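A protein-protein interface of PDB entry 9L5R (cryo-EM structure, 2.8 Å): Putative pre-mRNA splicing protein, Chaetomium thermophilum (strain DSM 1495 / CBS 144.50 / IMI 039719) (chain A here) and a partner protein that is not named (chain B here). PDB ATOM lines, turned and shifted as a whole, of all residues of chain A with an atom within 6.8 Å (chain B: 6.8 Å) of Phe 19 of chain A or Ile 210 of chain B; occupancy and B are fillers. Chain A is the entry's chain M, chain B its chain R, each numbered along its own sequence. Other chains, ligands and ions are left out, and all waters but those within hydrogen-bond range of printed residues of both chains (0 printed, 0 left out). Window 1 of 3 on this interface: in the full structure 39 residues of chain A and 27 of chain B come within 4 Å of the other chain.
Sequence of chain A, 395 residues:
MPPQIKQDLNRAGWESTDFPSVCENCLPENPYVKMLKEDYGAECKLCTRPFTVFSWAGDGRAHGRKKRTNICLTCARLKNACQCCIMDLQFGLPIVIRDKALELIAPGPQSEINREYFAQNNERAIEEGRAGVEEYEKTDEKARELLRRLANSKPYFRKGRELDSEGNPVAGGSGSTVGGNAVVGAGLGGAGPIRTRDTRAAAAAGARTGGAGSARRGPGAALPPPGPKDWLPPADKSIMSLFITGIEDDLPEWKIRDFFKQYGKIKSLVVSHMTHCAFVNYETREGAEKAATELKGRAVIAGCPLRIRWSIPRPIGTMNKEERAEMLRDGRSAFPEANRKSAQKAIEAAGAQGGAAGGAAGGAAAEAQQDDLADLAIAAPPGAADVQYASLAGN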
ATOM      1  N   ASP A  18       5.987  25.800   8.093  1.00  0.00           N
ATOM      2  CA  ASP A  18       6.654  26.567   7.051  1.00  0.00           C
ATOM      3  C   ASP A  18       7.912  25.877   6.559  1.00  0.00           C
ATOM      4  O   ASP A  18       8.675  26.450   5.792  1.00  0.00           O
ATOM      5  CB  ASP A  18       7.011  27.967   7.551  1.00  0.00           C
ATOM      6  CG  ASP A  18       5.884  28.959   7.359  1.00  0.00           C
ATOM      7  OD1 ASP A  18       4.920  28.639   6.630  1.00  0.00           O
ATOM      8  OD2 ASP A  18       5.974  30.067   7.922  1.00  0.00           O
ATOM      9  N   PHE A  19       8.133  24.646   7.017  1.00  0.00           N
ATOM     10  CA  PHE A  19       9.321  23.903   6.659  1.00  0.00           C
ATOM     11  C   PHE A  19       8.880  22.467   6.392  1.00  0.00           C
ATOM     12  O   PHE A  19       8.082  21.918   7.168  1.00  0.00           O
ATOM     13  CB  PHE A  19      10.387  23.962   7.762  1.00  0.00           C
ATOM     14  CG  PHE A  19      11.604  23.164   7.455  1.00  0.00           C
ATOM     15  CD1 PHE A  19      12.548  23.633   6.568  1.00  0.00           C
ATOM     16  CD2 PHE A  19      11.797  21.931   8.035  1.00  0.00           C
ATOM     17  CE1 PHE A  19      13.646  22.887   6.261  1.00  0.00           C
ATOM     18  CE2 PHE A  19      12.904  21.181   7.731  1.00  0.00           C
ATOM     19  CZ  PHE A  19      13.827  21.659   6.842  1.00  0.00           C
ATOM     20  N   PRO A  20       9.358  21.842   5.321  1.00  0.00           N
ATOM     21  CA  PRO A  20       8.868  20.514   4.958  1.00  0.00           C
ATOM     22  C   PRO A  20       9.306  19.429   5.930  1.00  0.00           C
ATOM     23  O   PRO A  20      10.310  19.542   6.633  1.00  0.00           O
ATOM     24  CB  PRO A  20       9.487  20.293   3.578  1.00  0.00           C
ATOM     25  CG  PRO A  20      10.698  21.103   3.600  1.00  0.00           C
ATOM     26  CD  PRO A  20      10.295  22.344   4.309  1.00  0.00           C
ATOM     27  N   SER A  21       8.524  18.353   5.959  1.00  0.00           N
ATOM     28  CA  SER A  21       8.870  17.160   6.727  1.00  0.00           C
ATOM     29  C   SER A  21       9.430  16.120   5.764  1.00  0.00           C
ATOM     30  O   SER A  21       8.756  15.188   5.348  1.00  0.00           O
ATOM     31  CB  SER A  21       7.663  16.642   7.484  1.00  0.00           C
ATOM     32  OG  SER A  21       7.460  17.403   8.653  1.00  0.00           O
ATOM     33  N   VAL A  22      10.701  16.285   5.432  1.00  0.00           N
ATOM     34  CA  VAL A  22      11.385  15.441   4.466  1.00  0.00           C
ATOM     35  C   VAL A  22      12.496  14.691   5.179  1.00  0.00           C
ATOM     36  O   VAL A  22      13.212  15.263   6.006  1.00  0.00           O
ATOM     37  CB  VAL A  22      11.940  16.270   3.292  1.00  0.00           C
ATOM     38  CG1 VAL A  22      12.527  15.375   2.256  1.00  0.00           C
ATOM     39  CG2 VAL A  22      10.840  17.074   2.673  1.00  0.00           C
ATOM     40  N   LEU A  27      16.528  14.169   1.432  1.00  0.00           N
ATOM     41  CA  LEU A  27      17.327  15.382   1.465  1.00  0.00           C
ATOM     42  C   LEU A  27      18.685  15.136   0.805  1.00  0.00           C
ATOM     43  O   LEU A  27      19.132  13.994   0.700  1.00  0.00           O
ATOM     44  CB  LEU A  27      17.496  15.846   2.911  1.00  0.00           C
ATOM     45  CG  LEU A  27      16.325  16.628   3.502  1.00  0.00           C
ATOM     46  CD1 LEU A  27      16.671  17.170   4.869  1.00  0.00           C
ATOM     47  CD2 LEU A  27      15.915  17.752   2.584  1.00  0.00           C
ATOM     48  N   VAL A  33      21.453  23.134   2.127  1.00  0.00           N
ATOM     49  CA  VAL A  33      20.387  22.818   1.188  1.00  0.00           C
ATOM     50  C   VAL A  33      19.861  24.105   0.571  1.00  0.00           C
ATOM     51  O   VAL A  33      19.619  25.091   1.273  1.00  0.00           O
ATOM     52  CB  VAL A  33      19.268  22.020   1.872  1.00  0.00           C
ATOM     53  CG1 VAL A  33      18.144  21.711   0.904  1.00  0.00           C
ATOM     54  CG2 VAL A  33      19.837  20.740   2.439  1.00  0.00           C
ATOM     55  N   LYS A  34      19.720  24.090  -0.747  1.00  0.00           N
ATOM     56  CA  LYS A  34      19.075  25.142  -1.517  1.00  0.00           C
ATOM     57  C   LYS A  34      17.672  24.660  -1.892  1.00  0.00           C
ATOM     58  O   LYS A  34      17.509  23.883  -2.834  1.00  0.00           O
ATOM     59  CB  LYS A  34      19.913  25.453  -2.751  1.00  0.00           C
ATOM     60  CG  LYS A  34      21.145  26.280  -2.496  1.00  0.00           C
ATOM     61  CD  LYS A  34      22.276  25.837  -3.388  1.00  0.00           C
ATOM     62  CE  LYS A  34      22.239  26.524  -4.725  1.00  0.00           C
ATOM     63  NZ  LYS A  34      23.118  25.870  -5.718  1.00  0.00           N
ATOM     64  N   MET A  35      16.660  25.109  -1.156  1.00  0.00           N
ATOM     65  CA  MET A  35      15.278  24.795  -1.495  1.00  0.00           C
ATOM     66  C   MET A  35      14.561  25.942  -2.179  1.00  0.00           C
ATOM     67  O   MET A  35      14.789  27.115  -1.887  1.00  0.00           O
ATOM     68  CB  MET A  35      14.425  24.395  -0.290  1.00  0.00           C
ATOM     69  CG  MET A  35      14.754  23.103   0.360  1.00  0.00           C
ATOM     70  SD  MET A  35      13.636  22.831   1.733  1.00  0.00           S
ATOM     71  CE  MET A  35      14.294  21.306   2.365  1.00  0.00           C
ATOM     72  N   LEU A  36      13.668  25.571  -3.081  1.00  0.00           N
ATOM     73  CA  LEU A  36      12.678  26.451  -3.666  1.00  0.00           C
ATOM     74  C   LEU A  36      11.339  26.191  -3.003  1.00  0.00           C
ATOM     75  O   LEU A  36      10.980  25.043  -2.743  1.00  0.00           O
ATOM     76  CB  LEU A  36      12.570  26.214  -5.167  1.00  0.00           C
ATOM     77  CG  LEU A  36      13.727  26.750  -5.994  1.00  0.00           C
ATOM     78  CD1 LEU A  36      13.893  25.929  -7.227  1.00  0.00           C
ATOM     79  CD2 LEU A  36      13.452  28.181  -6.354  1.00  0.00           C
ATOM     80  N   LYS A  37      10.614  27.256  -2.718  1.00  0.00           N
ATOM     81  CA  LYS A  37       9.309  27.174  -2.092  1.00  0.00           C
ATOM     82  C   LYS A  37       8.292  27.856  -2.990  1.00  0.00           C
ATOM     83  O   LYS A  37       8.510  28.985  -3.427  1.00  0.00           O
ATOM     84  CB  LYS A  37       9.340  27.832  -0.721  1.00  0.00           C
ATOM     85  CG  LYS A  37       8.014  27.957  -0.058  1.00  0.00           C
ATOM     86  CD  LYS A  37       8.148  28.799   1.161  1.00  0.00           C
ATOM     87  CE  LYS A  37       6.931  29.639   1.366  1.00  0.00           C
ATOM     88  NZ  LYS A  37       6.700  29.895   2.804  1.00  0.00           N
ATOM     89  N   PHE A  54       7.926  22.358  -1.680  1.00  0.00           N
ATOM     90  CA  PHE A  54       9.344  22.581  -1.458  1.00  0.00           C
ATOM     91  C   PHE A  54      10.105  21.631  -2.363  1.00  0.00           C
ATOM     92  O   PHE A  54       9.797  20.440  -2.404  1.00  0.00           O
ATOM     93  CB  PHE A  54       9.721  22.340   0.000  1.00  0.00           C
ATOM     94  CG  PHE A  54       9.145  23.339   0.944  1.00  0.00           C
ATOM     95  CD1 PHE A  54       7.894  23.151   1.481  1.00  0.00           C
ATOM     96  CD2 PHE A  54       9.860  24.453   1.309  1.00  0.00           C
ATOM     97  CE1 PHE A  54       7.357  24.067   2.343  1.00  0.00           C
ATOM     98  CE2 PHE A  54       9.332  25.369   2.175  1.00  0.00           C
ATOM     99  CZ  PHE A  54       8.085  25.178   2.699  1.00  0.00           C
ATOM    100  N   LEU A  73       1.485  18.719   4.289  1.00  0.00           N
ATOM    101  CA  LEU A  73       1.914  18.482   5.659  1.00  0.00           C
ATOM    102  C   LEU A  73       0.817  17.833   6.484  1.00  0.00           C
ATOM    103  O   LEU A  73       1.110  17.054   7.392  1.00  0.00           O
ATOM    104  CB  LEU A  73       2.352  19.791   6.304  1.00  0.00           C
ATOM    105  CG  LEU A  73       3.333  19.650   7.462  1.00  0.00           C
ATOM    106  CD1 LEU A  73       4.696  19.221   6.952  1.00  0.00           C
ATOM    107  CD2 LEU A  73       3.428  20.953   8.238  1.00  0.00           C
ATOM    108  N   GLN A  83       7.401  13.491   3.293  1.00  0.00           N
ATOM    109  CA  GLN A  83       6.603  14.310   2.409  1.00  0.00           C
ATOM    110  C   GLN A  83       7.064  14.215   0.959  1.00  0.00           C
ATOM    111  O   GLN A  83       6.295  14.551   0.059  1.00  0.00           O
ATOM    112  CB  GLN A  83       6.630  15.725   2.965  1.00  0.00           C
ATOM    113  CG  GLN A  83       5.635  16.625   2.414  1.00  0.00           C
ATOM    114  CD  GLN A  83       5.533  17.909   3.177  1.00  0.00           C
ATOM    115  OE1 GLN A  83       6.249  18.126   4.141  1.00  0.00           O
ATOM    116  NE2 GLN A  83       4.632  18.770   2.752  1.00  0.00           N
ATOM    117  N   GLU B 185      14.390  37.776  -1.121  1.00  0.00           N
ATOM    118  CA  GLU B 185      15.500  37.329  -0.292  1.00  0.00           C
ATOM    119  C   GLU B 185      15.254  35.915   0.225  1.00  0.00           C
ATOM    120  O   GLU B 185      14.158  35.361   0.118  1.00  0.00           O
ATOM    121  CB  GLU B 185      15.732  38.284   0.881  1.00  0.00           C
ATOM    122  CG  GLU B 185      14.631  38.272   1.935  1.00  0.00           C
ATOM    123  CD  GLU B 185      13.467  39.193   1.600  1.00  0.00           C
ATOM    124  OE1 GLU B 185      13.350  39.619   0.440  1.00  0.00           O
ATOM    125  OE2 GLU B 185      12.663  39.495   2.502  1.00  0.00           O
ATOM    126  N   ALA B 186      16.300  35.333   0.794  1.00  0.00           N
ATOM    127  CA  ALA B 186      16.294  33.954   1.244  1.00  0.00           C
ATOM    128  C   ALA B 186      16.106  33.878   2.751  1.00  0.00           C
ATOM    129  O   ALA B 186      16.588  34.726   3.503  1.00  0.00           O
ATOM    130  CB  ALA B 186      17.594  33.255   0.863  1.00  0.00           C
ATOM    131  N   THR B 187      15.393  32.846   3.182  1.00  0.00           N
ATOM    132  CA  THR B 187      15.297  32.478   4.582  1.00  0.00           C
ATOM    133  C   THR B 187      16.308  31.372   4.850  1.00  0.00           C
ATOM    134  O   THR B 187      16.564  30.535   3.983  1.00  0.00           O
ATOM    135  CB  THR B 187      13.877  32.011   4.909  1.00  0.00           C
ATOM    136  OG1 THR B 187      12.958  33.071   4.637  1.00  0.00           O
ATOM    137  CG2 THR B 187      13.726  31.607   6.360  1.00  0.00           C
ATOM    138  N   PHE B 188      16.918  31.392   6.028  1.00  0.00           N
ATOM    139  CA  PHE B 188      17.785  30.311   6.459  1.00  0.00           C
ATOM    140  C   PHE B 188      17.146  29.590   7.637  1.00  0.00           C
ATOM    141  O   PHE B 188      16.546  30.219   8.510  1.00  0.00           O
ATOM    142  CB  PHE B 188      19.170  30.836   6.822  1.00  0.00           C
ATOM    143  CG  PHE B 188      19.976  31.267   5.635  1.00  0.00           C
ATOM    144  CD1 PHE B 188      20.568  30.334   4.810  1.00  0.00           C
ATOM    145  CD2 PHE B 188      20.127  32.607   5.332  1.00  0.00           C
ATOM    146  CE1 PHE B 188      21.298  30.724   3.718  1.00  0.00           C
ATOM    147  CE2 PHE B 188      20.862  32.998   4.240  1.00  0.00           C
ATOM    148  CZ  PHE B 188      21.450  32.053   3.435  1.00  0.00           C
ATOM    149  N   VAL B 189      17.246  28.267   7.635  1.00  0.00           N
ATOM    150  CA  VAL B 189      16.644  27.418   8.658  1.00  0.00           C
ATOM    151  C   VAL B 189      17.736  26.507   9.201  1.00  0.00           C
ATOM    152  O   VAL B 189      18.524  25.947   8.437  1.00  0.00           O
ATOM    153  CB  VAL B 189      15.449  26.613   8.095  1.00  0.00           C
ATOM    154  CG1 VAL B 189      15.051  25.490   9.015  1.00  0.00           C
ATOM    155  CG2 VAL B 189      14.259  27.521   7.871  1.00  0.00           C
ATOM    156  N   TYR B 191      17.819  23.599  11.018  1.00  0.00           N
ATOM    157  CA  TYR B 191      17.477  22.177  10.876  1.00  0.00           C
ATOM    158  C   TYR B 191      18.283  21.129  11.642  1.00  0.00           C
ATOM    159  O   TYR B 191      19.160  20.481  11.064  1.00  0.00           O
ATOM    160  CB  TYR B 191      17.441  21.741   9.420  1.00  0.00           C
ATOM    161  CG  TYR B 191      16.637  20.461   9.291  1.00  0.00           C
ATOM    162  CD1 TYR B 191      15.454  20.288  10.004  1.00  0.00           C
ATOM    163  CD2 TYR B 191      17.074  19.419   8.496  1.00  0.00           C
ATOM    164  CE1 TYR B 191      14.728  19.124   9.907  1.00  0.00           C
ATOM    165  CE2 TYR B 191      16.354  18.260   8.395  1.00  0.00           C
ATOM    166  CZ  TYR B 191      15.189  18.116   9.103  1.00  0.00           C
ATOM    167  OH  TYR B 191      14.485  16.950   8.984  1.00  0.00           O
ATOM    168  N   ARG B 206      21.754  20.664   9.771  1.00  0.00           N
ATOM    169  CA  ARG B 206      21.482  21.086   8.399  1.00  0.00           C
ATOM    170  C   ARG B 206      21.027  22.536   8.311  1.00  0.00           C
ATOM    171  O   ARG B 206      20.033  22.931   8.943  1.00  0.00           O
ATOM    172  CB  ARG B 206      20.436  20.179   7.758  1.00  0.00           C
ATOM    173  CG  ARG B 206      21.017  18.995   7.055  1.00  0.00           C
ATOM    174  CD  ARG B 206      20.051  18.465   6.049  1.00  0.00           C
ATOM    175  NE  ARG B 206      20.358  17.093   5.680  1.00  0.00           N
ATOM    176  CZ  ARG B 206      20.907  16.749   4.527  1.00  0.00           C
ATOM    177  NH1 ARG B 206      21.253  17.653   3.634  1.00  0.00           N
ATOM    178  NH2 ARG B 206      21.112  15.465   4.262  1.00  0.00           N
ATOM    179  N   ILE B 208      19.400  25.215   5.826  1.00  0.00           N
ATOM    180  CA  ILE B 208      18.506  25.201   4.677  1.00  0.00           C
ATOM    181  C   ILE B 208      18.372  26.630   4.172  1.00  0.00           C
ATOM    182  O   ILE B 208      18.051  27.534   4.949  1.00  0.00           O
ATOM    183  CB  ILE B 208      17.122  24.642   5.041  1.00  0.00           C
ATOM    184  CG1 ILE B 208      17.219  23.361   5.874  1.00  0.00           C
ATOM    185  CG2 ILE B 208      16.361  24.325   3.778  1.00  0.00           C
ATOM    186  CD1 ILE B 208      17.864  22.212   5.204  1.00  0.00           C
ATOM    187  N   LYS B 209      18.612  26.831   2.880  1.00  0.00           N
ATOM    188  CA  LYS B 209      18.379  28.111   2.218  1.00  0.00           C
ATOM    189  C   LYS B 209      17.101  27.999   1.399  1.00  0.00           C
ATOM    190  O   LYS B 209      17.079  27.325   0.369  1.00  0.00           O
ATOM    191  CB  LYS B 209      19.555  28.486   1.323  1.00  0.00           C
ATOM    192  CG  LYS B 209      19.425  29.850   0.702  1.00  0.00           C
ATOM    193  CD  LYS B 209      20.708  30.280   0.065  1.00  0.00           C
ATOM    194  CE  LYS B 209      20.456  31.144  -1.145  1.00  0.00           C
ATOM    195  NZ  LYS B 209      21.687  31.272  -1.952  1.00  0.00           N
ATOM    196  N   ILE B 210      16.048  28.673   1.837  1.00  0.00           N
ATOM    197  CA  ILE B 210      14.747  28.599   1.193  1.00  0.00           C
ATOM    198  C   ILE B 210      14.490  29.918   0.488  1.00  0.00           C
ATOM    199  O   ILE B 210      14.487  30.979   1.122  1.00  0.00           O
ATOM    200  CB  ILE B 210      13.628  28.296   2.201  1.00  0.00           C
ATOM    201  CG1 ILE B 210      13.982  27.069   3.040  1.00  0.00           C
ATOM    202  CG2 ILE B 210      12.318  28.092   1.483  1.00  0.00           C
ATOM    203  CD1 ILE B 210      12.933  26.693   4.041  1.00  0.00           C
ATOM    204  N   VAL B 211      14.268  29.855  -0.822  1.00  0.00           N
ATOM    205  CA  VAL B 211      13.855  31.012  -1.603  1.00  0.00           C
ATOM    206  C   VAL B 211      12.500  30.719  -2.232  1.00  0.00           C
ATOM    207  O   VAL B 211      12.164  29.571  -2.530  1.00  0.00           O
ATOM    208  CB  VAL B 211      14.904  31.399  -2.676  1.00  0.00           C
ATOM    209  CG1 VAL B 211      16.263  31.488  -2.060  1.00  0.00           C
ATOM    210  CG2 VAL B 211      14.945  30.396  -3.798  1.00  0.00           C
ATOM    211  N   GLU B 212      11.691  31.763  -2.367  1.00  0.00           N
ATOM    212  CA  GLU B 212      10.441  31.665  -3.104  1.00  0.00           C
ATOM    213  C   GLU B 212      10.735  31.593  -4.596  1.00  0.00           C
ATOM    214  O   GLU B 212      11.566  32.335  -5.113  1.00  0.00           O
ATOM    215  CB  GLU B 212       9.553  32.863  -2.778  1.00  0.00           C
ATOM    216  CG  GLU B 212       8.149  32.800  -3.330  1.00  0.00           C
ATOM    217  CD  GLU B 212       7.438  34.142  -3.271  1.00  0.00           C
ATOM    218  OE1 GLU B 212       7.319  34.707  -2.166  1.00  0.00           O
ATOM    219  OE2 GLU B 212       7.003  34.647  -4.328  1.00  0.00           O
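N of Lys 37 of chain A sits at hydrogen-bond distance from O of Val 211 of chain B (2.8 Å).
The backbone carbonyl oxygen of Val 33 of chain A lies within hydrogen-bond range of the backbone NH of Lys 209 of chain B (2.6 Å).
The backbone NH (N) of Val 211 of chain B sits at hydrogen-bond distance from the backbone carbonyl oxygen (O) of Met 35 of chain A (3.0 Å).
N of Met 35 of chain A is in hydrogen-bond range of O of Lys 209 of chain B (2.7 Å).
N of Arg 206 of chain B lies within hydrogen-bond range of O of Tyr 191 of chain B (2.9 Å).
The backbone NH of Ile 210 of chain B lies within hydrogen-bond range of the backbone carbonyl oxygen of Thr 187 of chain B (2.9 Å).
The backbone NH (N) of Ile 208 of chain B is in hydrogen-bond range of the backbone carbonyl oxygen (O) of Val 189 of chain B.
Val 189 of chain B touches Phe 19 of chain A.
Phe 19 of chain A touches Tyr 191 of chain B (CE2 to CE1, 3.5 Å).
Phe 19 of chain A touches Ile 208 of chain B.
Phe 19 of chain A touches Ile 210 of chain B.
Leu 27 of chain A touches Arg 206 of chain B.
Val 33 of chain A touches Arg 206 of chain B.
Lys 209 of chain B touches Lys 34 of chain A (O to CA, 3.5 Å).
Ile 208 of chain B touches Met 35 of chain A (CG2 to SD, 3.7 Å).
Met 35 of chain A touches Ile 210 of chain B (O to CA, 3.4 Å).
Val 211 of chain B touches Leu 36 of chain A.
Of the printed residues of chain B, Phe 19 of chain A touches Val 189, Tyr 191, Ile 208 and Ile 210.
Of the printed residues of chain B, Leu 27 of chain A touches Tyr 191 and Arg 206.
Of the printed residues of chain B, Lys 34 of chain A touches Lys 209 (3.5 Å).
Of the printed residues of chain A, Arg 206 of chain B touches Leu 27 and Val 33.
Of the printed residues of chain A, Ile 210 of chain B touches Phe 19, Met 35 and Lys 37.
Of the printed residues of chain A, Glu 212 of chain B touches Lys 37 (3.3 Å).
The nearest printed residue of chain A that does not touch Ile 210 of chain B is Phe 54 of chain A (4.1 Å).
Hydrophobic or aromatic side chains of chain A that line the printed part of chain B: Phe 19, Leu 27, Val 33, Met 35 and Leu 36.
Hydrophobic or aromatic side chains of chain B that line the printed part of chain A: Val 189, Tyr 191, Ile 208, Ile 210 and Val 211.
Among the printed residues, 19 pairs touch across the chains.
Among the printed residues, no Asp or Glu carboxylate lies within 4 Å of a Lys or Arg side-chain nitrogen of the other chain.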
